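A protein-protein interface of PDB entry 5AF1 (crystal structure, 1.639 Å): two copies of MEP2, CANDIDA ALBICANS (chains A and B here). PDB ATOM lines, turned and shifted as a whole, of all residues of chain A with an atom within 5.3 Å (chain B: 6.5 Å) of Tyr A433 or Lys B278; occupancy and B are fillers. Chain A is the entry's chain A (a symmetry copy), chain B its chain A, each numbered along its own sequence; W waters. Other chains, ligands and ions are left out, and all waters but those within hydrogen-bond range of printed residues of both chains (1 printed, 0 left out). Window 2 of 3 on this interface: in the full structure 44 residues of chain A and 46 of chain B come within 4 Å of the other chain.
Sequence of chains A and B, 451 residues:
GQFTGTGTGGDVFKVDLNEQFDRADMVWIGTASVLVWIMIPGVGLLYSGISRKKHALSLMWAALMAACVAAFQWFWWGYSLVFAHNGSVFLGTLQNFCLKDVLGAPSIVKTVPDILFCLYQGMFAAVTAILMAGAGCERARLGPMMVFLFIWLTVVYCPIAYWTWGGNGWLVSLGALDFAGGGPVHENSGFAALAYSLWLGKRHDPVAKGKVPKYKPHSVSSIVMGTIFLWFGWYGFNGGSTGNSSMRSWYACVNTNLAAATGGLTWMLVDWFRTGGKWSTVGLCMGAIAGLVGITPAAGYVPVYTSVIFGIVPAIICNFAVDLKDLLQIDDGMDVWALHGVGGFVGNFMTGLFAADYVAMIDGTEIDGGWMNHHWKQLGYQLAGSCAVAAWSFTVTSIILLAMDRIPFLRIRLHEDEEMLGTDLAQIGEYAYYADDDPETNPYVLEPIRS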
ATOM      1  N   GLU A 430     -29.272 -21.181 -15.941  1.00  0.00           N
ATOM      2  CA  GLU A 430     -29.759 -21.499 -17.278  1.00  0.00           C
ATOM      3  C   GLU A 430     -29.065 -20.650 -18.345  1.00  0.00           C
ATOM      4  O   GLU A 430     -29.035 -21.020 -19.519  1.00  0.00           O
ATOM      5  CB  GLU A 430     -31.277 -21.310 -17.363  1.00  0.00           C
ATOM      6  N   TYR A 431     -28.505 -19.515 -17.935  1.00  0.00           N
ATOM      7  CA  TYR A 431     -27.864 -18.599 -18.880  1.00  0.00           C
ATOM      8  C   TYR A 431     -26.357 -18.464 -18.647  1.00  0.00           C
ATOM      9  O   TYR A 431     -25.760 -17.445 -18.997  1.00  0.00           O
ATOM     10  CB  TYR A 431     -28.517 -17.217 -18.806  1.00  0.00           C
ATOM     11  CG  TYR A 431     -29.965 -17.189 -19.243  1.00  0.00           C
ATOM     12  CD1 TYR A 431     -30.309 -17.255 -20.588  1.00  0.00           C
ATOM     13  CD2 TYR A 431     -30.988 -17.084 -18.310  1.00  0.00           C
ATOM     14  CE1 TYR A 431     -31.632 -17.225 -20.990  1.00  0.00           C
ATOM     15  CE2 TYR A 431     -32.312 -17.051 -18.701  1.00  0.00           C
ATOM     16  CZ  TYR A 431     -32.630 -17.123 -20.041  1.00  0.00           C
ATOM     17  OH  TYR A 431     -33.949 -17.092 -20.430  1.00  0.00           O
ATOM     18  N   ALA A 432     -25.747 -19.498 -18.074  1.00  0.00           N
ATOM     19  CA  ALA A 432     -24.329 -19.453 -17.721  1.00  0.00           C
ATOM     20  C   ALA A 432     -23.417 -19.257 -18.935  1.00  0.00           C
ATOM     21  O   ALA A 432     -22.301 -18.757 -18.803  1.00  0.00           O
ATOM     22  CB  ALA A 432     -23.935 -20.720 -16.969  1.00  0.00           C
ATOM     23  N   TYR A 433     -23.898 -19.634 -20.116  1.00  0.00           N
ATOM     24  CA  TYR A 433     -23.101 -19.526 -21.339  1.00  0.00           C
ATOM     25  C   TYR A 433     -22.881 -18.076 -21.776  1.00  0.00           C
ATOM     26  O   TYR A 433     -22.100 -17.812 -22.689  1.00  0.00           O
ATOM     27  CB  TYR A 433     -23.747 -20.330 -22.478  1.00  0.00           C
ATOM     28  CG  TYR A 433     -25.167 -19.937 -22.838  1.00  0.00           C
ATOM     29  CD1 TYR A 433     -26.249 -20.370 -22.072  1.00  0.00           C
ATOM     30  CD2 TYR A 433     -25.432 -19.159 -23.960  1.00  0.00           C
ATOM     31  CE1 TYR A 433     -27.549 -20.020 -22.406  1.00  0.00           C
ATOM     32  CE2 TYR A 433     -26.727 -18.809 -24.304  1.00  0.00           C
ATOM     33  CZ  TYR A 433     -27.780 -19.243 -23.527  1.00  0.00           C
ATOM     34  OH  TYR A 433     -29.069 -18.893 -23.864  1.00  0.00           O
ATOM     35  N   TYR A 434     -23.557 -17.139 -21.117  1.00  0.00           N
ATOM     36  CA  TYR A 434     -23.353 -15.718 -21.394  1.00  0.00           C
ATOM     37  C   TYR A 434     -22.015 -15.215 -20.851  1.00  0.00           C
ATOM     38  O   TYR A 434     -21.586 -14.107 -21.173  1.00  0.00           O
ATOM     39  CB  TYR A 434     -24.512 -14.892 -20.820  1.00  0.00           C
ATOM     40  CG  TYR A 434     -25.649 -14.775 -21.805  1.00  0.00           C
ATOM     41  CD1 TYR A 434     -26.541 -15.824 -21.985  1.00  0.00           C
ATOM     42  CD2 TYR A 434     -25.814 -13.632 -22.577  1.00  0.00           C
ATOM     43  CE1 TYR A 434     -27.570 -15.736 -22.901  1.00  0.00           C
ATOM     44  CE2 TYR A 434     -26.842 -13.535 -23.502  1.00  0.00           C
ATOM     45  CZ  TYR A 434     -27.717 -14.592 -23.657  1.00  0.00           C
ATOM     46  OH  TYR A 434     -28.743 -14.518 -24.570  1.00  0.00           O
ATOM     47  N   ALA A 435     -21.357 -16.040 -20.039  1.00  0.00           N
ATOM     48  CA  ALA A 435     -20.054 -15.696 -19.479  1.00  0.00           C
ATOM     49  C   ALA A 435     -18.956 -15.697 -20.541  1.00  0.00           C
ATOM     50  O   ALA A 435     -17.916 -15.065 -20.368  1.00  0.00           O
ATOM     51  CB  ALA A 435     -19.696 -16.652 -18.356  1.00  0.00           C
ATOM     52  N   ASP A 436     -19.186 -16.417 -21.634  1.00  0.00           N
ATOM     53  CA  ASP A 436     -18.241 -16.440 -22.745  1.00  0.00           C
ATOM     54  C   ASP A 436     -18.685 -15.489 -23.852  1.00  0.00           C
ATOM     55  O   ASP A 436     -19.374 -15.896 -24.783  1.00  0.00           O
ATOM     56  CB  ASP A 436     -18.094 -17.862 -23.292  1.00  0.00           C
ATOM     57  N   ASN A 442     -17.761 -19.040 -28.885  1.00  0.00           N
ATOM     58  CA  ASN A 442     -19.111 -19.241 -28.364  1.00  0.00           C
ATOM     59  C   ASN A 442     -20.020 -19.805 -29.442  1.00  0.00           C
ATOM     60  O   ASN A 442     -20.152 -19.217 -30.515  1.00  0.00           O
ATOM     61  CB  ASN A 442     -19.703 -17.941 -27.812  1.00  0.00           C
ATOM     62  CG  ASN A 442     -20.831 -18.193 -26.817  1.00  0.00           C
ATOM     63  OD1 ASN A 442     -21.707 -19.027 -27.049  1.00  0.00           O
ATOM     64  ND2 ASN A 442     -20.798 -17.487 -25.688  1.00  0.00           N
ATOM     65  N   TYR A 444     -23.194 -19.975 -29.374  1.00  0.00           N
ATOM     66  CA  TYR A 444     -24.517 -19.356 -29.402  1.00  0.00           C
ATOM     67  C   TYR A 444     -24.446 -17.839 -29.471  1.00  0.00           C
ATOM     68  O   TYR A 444     -23.562 -17.219 -28.877  1.00  0.00           O
ATOM     69  CB  TYR A 444     -25.331 -19.804 -28.182  1.00  0.00           C
ATOM     70  CG  TYR A 444     -25.465 -21.311 -28.121  1.00  0.00           C
ATOM     71  CD1 TYR A 444     -26.169 -21.993 -29.100  1.00  0.00           C
ATOM     72  CD2 TYR A 444     -24.871 -22.050 -27.105  1.00  0.00           C
ATOM     73  CE1 TYR A 444     -26.294 -23.366 -29.072  1.00  0.00           C
ATOM     74  CE2 TYR A 444     -24.993 -23.433 -27.066  1.00  0.00           C
ATOM     75  CZ  TYR A 444     -25.706 -24.082 -28.056  1.00  0.00           C
ATOM     76  OH  TYR A 444     -25.839 -25.454 -28.041  1.00  0.00           O
ATOM     77  N   VAL A 445     -25.374 -17.250 -30.217  1.00  0.00           N
ATOM     78  CA  VAL A 445     -25.526 -15.806 -30.249  1.00  0.00           C
ATOM     79  C   VAL A 445     -25.893 -15.349 -28.842  1.00  0.00           C
ATOM     80  O   VAL A 445     -26.805 -15.905 -28.237  1.00  0.00           O
ATOM     81  CB  VAL A 445     -26.621 -15.365 -31.243  1.00  0.00           C
ATOM     82  CG1 VAL A 445     -26.749 -13.852 -31.268  1.00  0.00           C
ATOM     83  CG2 VAL A 445     -26.324 -15.900 -32.657  1.00  0.00           C
ATOM     84  N   LEU A 446     -25.173 -14.363 -28.313  1.00  0.00           N
ATOM     85  CA  LEU A 446     -25.499 -13.864 -26.984  1.00  0.00           C
ATOM     86  C   LEU A 446     -26.594 -12.815 -27.100  1.00  0.00           C
ATOM     87  O   LEU A 446     -26.382 -11.610 -26.964  1.00  0.00           O
ATOM     88  CB  LEU A 446     -24.263 -13.321 -26.277  1.00  0.00           C
ATOM     89  CG  LEU A 446     -23.304 -14.460 -25.925  1.00  0.00           C
ATOM     90  CD1 LEU A 446     -22.276 -14.000 -24.914  1.00  0.00           C
ATOM     91  CD2 LEU A 446     -24.064 -15.683 -25.410  1.00  0.00           C
ATOM     92  N   MET B 268     -30.529 -24.111 -38.118  1.00  0.00           N
ATOM     93  CA  MET B 268     -30.548 -23.172 -36.997  1.00  0.00           C
ATOM     94  C   MET B 268     -31.893 -23.220 -36.260  1.00  0.00           C
ATOM     95  O   MET B 268     -31.949 -23.166 -35.033  1.00  0.00           O
ATOM     96  CB  MET B 268     -30.235 -21.750 -37.476  1.00  0.00           C
ATOM     97  CG  MET B 268     -30.014 -20.800 -36.300  1.00  0.00           C
ATOM     98  SD  MET B 268     -29.366 -19.208 -36.835  1.00  0.00           S
ATOM     99  CE  MET B 268     -30.799 -18.496 -37.637  1.00  0.00           C
ATOM    100  N   ASP B 271     -31.936 -26.374 -34.126  1.00  0.00           N
ATOM    101  CA  ASP B 271     -31.144 -26.153 -32.907  1.00  0.00           C
ATOM    102  C   ASP B 271     -31.922 -25.287 -31.917  1.00  0.00           C
ATOM    103  O   ASP B 271     -31.875 -25.507 -30.710  1.00  0.00           O
ATOM    104  CB  ASP B 271     -29.808 -25.478 -33.217  1.00  0.00           C
ATOM    105  CG  ASP B 271     -28.755 -26.441 -33.741  1.00  0.00           C
ATOM    106  OD1 ASP B 271     -28.901 -27.670 -33.574  1.00  0.00           O
ATOM    107  OD2 ASP B 271     -27.766 -25.949 -34.322  1.00  0.00           O
ATOM    108  N   TRP B 272     -32.635 -24.295 -32.437  1.00  0.00           N
ATOM    109  CA  TRP B 272     -33.431 -23.394 -31.605  1.00  0.00           C
ATOM    110  C   TRP B 272     -34.482 -24.172 -30.813  1.00  0.00           C
ATOM    111  O   TRP B 272     -34.640 -23.989 -29.595  1.00  0.00           O
ATOM    112  CB  TRP B 272     -34.083 -22.327 -32.493  1.00  0.00           C
ATOM    113  CG  TRP B 272     -34.863 -21.290 -31.749  1.00  0.00           C
ATOM    114  CD1 TRP B 272     -34.378 -20.129 -31.210  1.00  0.00           C
ATOM    115  CD2 TRP B 272     -36.266 -21.307 -31.472  1.00  0.00           C
ATOM    116  NE1 TRP B 272     -35.395 -19.427 -30.612  1.00  0.00           N
ATOM    117  CE2 TRP B 272     -36.564 -20.127 -30.761  1.00  0.00           C
ATOM    118  CE3 TRP B 272     -37.301 -22.203 -31.759  1.00  0.00           C
ATOM    119  CZ2 TRP B 272     -37.852 -19.826 -30.324  1.00  0.00           C
ATOM    120  CZ3 TRP B 272     -38.578 -21.900 -31.328  1.00  0.00           C
ATOM    121  CH2 TRP B 272     -38.843 -20.721 -30.617  1.00  0.00           C
ATOM    122  N   PHE B 273     -35.183 -25.068 -31.500  1.00  0.00           N
ATOM    123  CA  PHE B 273     -36.168 -25.911 -30.834  1.00  0.00           C
ATOM    124  C   PHE B 273     -35.519 -26.862 -29.831  1.00  0.00           C
ATOM    125  O   PHE B 273     -36.015 -27.015 -28.717  1.00  0.00           O
ATOM    126  CB  PHE B 273     -36.980 -26.707 -31.852  1.00  0.00           C
ATOM    127  CG  PHE B 273     -38.086 -25.924 -32.481  1.00  0.00           C
ATOM    128  CD1 PHE B 273     -39.217 -25.593 -31.749  1.00  0.00           C
ATOM    129  CD2 PHE B 273     -38.005 -25.518 -33.801  1.00  0.00           C
ATOM    130  CE1 PHE B 273     -40.246 -24.867 -32.327  1.00  0.00           C
ATOM    131  CE2 PHE B 273     -39.031 -24.792 -34.384  1.00  0.00           C
ATOM    132  CZ  PHE B 273     -40.151 -24.467 -33.646  1.00  0.00           C
ATOM    133  N   THR B 275     -32.605 -26.688 -28.249  1.00  0.00           N
ATOM    134  CA  THR B 275     -31.908 -26.038 -27.136  1.00  0.00           C
ATOM    135  C   THR B 275     -32.832 -25.198 -26.263  1.00  0.00           C
ATOM    136  O   THR B 275     -32.392 -24.597 -25.288  1.00  0.00           O
ATOM    137  CB  THR B 275     -30.788 -25.108 -27.622  1.00  0.00           C
ATOM    138  OG1 THR B 275     -31.356 -24.068 -28.431  1.00  0.00           O
ATOM    139  CG2 THR B 275     -29.734 -25.876 -28.419  1.00  0.00           C
ATOM    140  N   GLY B 276     -34.105 -25.128 -26.624  1.00  0.00           N
ATOM    141  CA  GLY B 276     -35.042 -24.319 -25.869  1.00  0.00           C
ATOM    142  C   GLY B 276     -34.836 -22.828 -26.057  1.00  0.00           C
ATOM    143  O   GLY B 276     -35.073 -22.043 -25.141  1.00  0.00           O
ATOM    144  N   GLY B 277     -34.371 -22.435 -27.237  1.00  0.00           N
ATOM    145  CA  GLY B 277     -34.360 -21.032 -27.608  1.00  0.00           C
ATOM    146  C   GLY B 277     -33.024 -20.381 -27.922  1.00  0.00           C
ATOM    147  O   GLY B 277     -32.964 -19.163 -28.084  1.00  0.00           O
ATOM    148  N   LYS B 278     -31.958 -21.173 -28.032  1.00  0.00           N
ATOM    149  CA  LYS B 278     -30.650 -20.610 -28.364  1.00  0.00           C
ATOM    150  C   LYS B 278     -30.469 -20.498 -29.867  1.00  0.00           C
ATOM    151  O   LYS B 278     -31.015 -21.302 -30.624  1.00  0.00           O
ATOM    152  CB  LYS B 278     -29.516 -21.457 -27.786  1.00  0.00           C
ATOM    153  CG  LYS B 278     -29.565 -21.665 -26.276  1.00  0.00           C
ATOM    154  CD  LYS B 278     -28.376 -22.516 -25.840  1.00  0.00           C
ATOM    155  CE  LYS B 278     -28.398 -22.822 -24.350  1.00  0.00           C
ATOM    156  NZ  LYS B 278     -29.546 -23.691 -23.965  1.00  0.00           N
ATOM    157  N   TRP B 279     -29.690 -19.506 -30.292  1.00  0.00           N
ATOM    158  CA  TRP B 279     -29.365 -19.332 -31.703  1.00  0.00           C
ATOM    159  C   TRP B 279     -27.960 -19.848 -31.987  1.00  0.00           C
ATOM    160  O   TRP B 279     -26.967 -19.293 -31.508  1.00  0.00           O
ATOM    161  CB  TRP B 279     -29.486 -17.866 -32.113  1.00  0.00           C
ATOM    162  CG  TRP B 279     -30.892 -17.373 -32.083  1.00  0.00           C
ATOM    163  CD1 TRP B 279     -31.408 -16.421 -31.255  1.00  0.00           C
ATOM    164  CD2 TRP B 279     -31.972 -17.808 -32.920  1.00  0.00           C
ATOM    165  NE1 TRP B 279     -32.744 -16.236 -31.523  1.00  0.00           N
ATOM    166  CE2 TRP B 279     -33.114 -17.075 -32.541  1.00  0.00           C
ATOM    167  CE3 TRP B 279     -32.085 -18.748 -33.954  1.00  0.00           C
ATOM    168  CZ2 TRP B 279     -34.354 -17.248 -33.159  1.00  0.00           C
ATOM    169  CZ3 TRP B 279     -33.316 -18.919 -34.563  1.00  0.00           C
ATOM    170  CH2 TRP B 279     -34.431 -18.171 -34.164  1.00  0.00           C
ATOM    171  N   SER B 280     -27.900 -20.921 -32.768  1.00  0.00           N
ATOM    172  CA  SER B 280     -26.675 -21.681 -32.998  1.00  0.00           C
ATOM    173  C   SER B 280     -25.852 -21.139 -34.165  1.00  0.00           C
ATOM    174  O   SER B 280     -26.244 -21.285 -35.318  1.00  0.00           O
ATOM    175  CB  SER B 280     -27.034 -23.145 -33.263  1.00  0.00           C
ATOM    176  OG  SER B 280     -25.894 -23.937 -33.529  1.00  0.00           O
HETATM  177  O   HOH W   1     -28.642 -17.743 -28.343  1.00  0.00           O
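N of Val A445 is in hydrogen-bond range of O of Trp B279 (2.9 Å).
O of Asp B271 is in hydrogen-bond range of OG1 of Thr B275, 2.7 Å away. OG of Ser B280 lies within hydrogen-bond range of OD2 of Asp B271 (2.9 Å). The backbone carbonyl oxygen of Trp B272 is in hydrogen-bond range of the side-chain hydroxyl of Thr B275, 3.5 Å away. N of Lys B278 is in hydrogen-bond range of OG1 of Thr B275, at 3.0 Å. The backbone carbonyl oxygen of Tyr A433 sits at hydrogen-bond distance from the side-chain amide nitrogen of Asn A442. The side-chain amide oxygen (OD1) of Asn A442 sits at hydrogen-bond distance from the backbone NH (N) of Tyr A444 (2.9 Å).
Lys B278 touches Tyr A433 (CE to CE1, 3.5 Å). OH of Tyr A444 touches CG2 of Thr B275, 3.9 Å away. Tyr A444 touches Lys B278 (CD1 to CB, 3.6 Å). CA of Tyr A444 touches O of Trp B279, 3.2 Å away. Ser B280 touches Tyr A444.
Glu A430 touches none of the printed residues of chain B. Tyr A433 touches just one residue of chain B: Lys B278 (3.5 Å). Of the printed residues of chain B, Tyr A444 touches Thr B275 (3.9 Å), Lys B278 (3.6 Å), Trp B279 (3.2 Å) and Ser B280 (3.9 Å). Asp B271 touches none of the printed residues of chain A. Lys B278 touches just these residues of chain A: Tyr A433 (3.5 Å) and Tyr A444 (3.6 Å). Of the printed residues of chain A, Trp B279 touches Tyr A444 (3.2 Å) and Val A445 (2.9 Å). The nearest residue of chain B that does not touch Tyr A433 is Gly B277 (5.7 Å). The nearest residue of chain A that does not touch Lys B278 is Glu A430 (5.2 Å). The nearest printed residue of chain B that does not touch Val A445 is Ser B280 (5.1 Å).
Hydrophobic or aromatic side chains of chain B that line the printed part of chain A: Trp B279. Hydrophobic or aromatic side chains of chain A within 4 Å of the printed part of chain B: Tyr A433, Tyr A444 and Val A445. Along chain A the printed residues that touch a printed residue of chain B span positions 433 to 445. Among the printed residues, 6 pairs touch across the chains.
No position is printed for both chains. Of the 6 pairs that touch across the chains among the printed residues, none has its exchanged pair printed and touching as well.
Water W1 bridges O of Val A445 (2.6 Å) and N of Trp B279 (2.8 Å).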
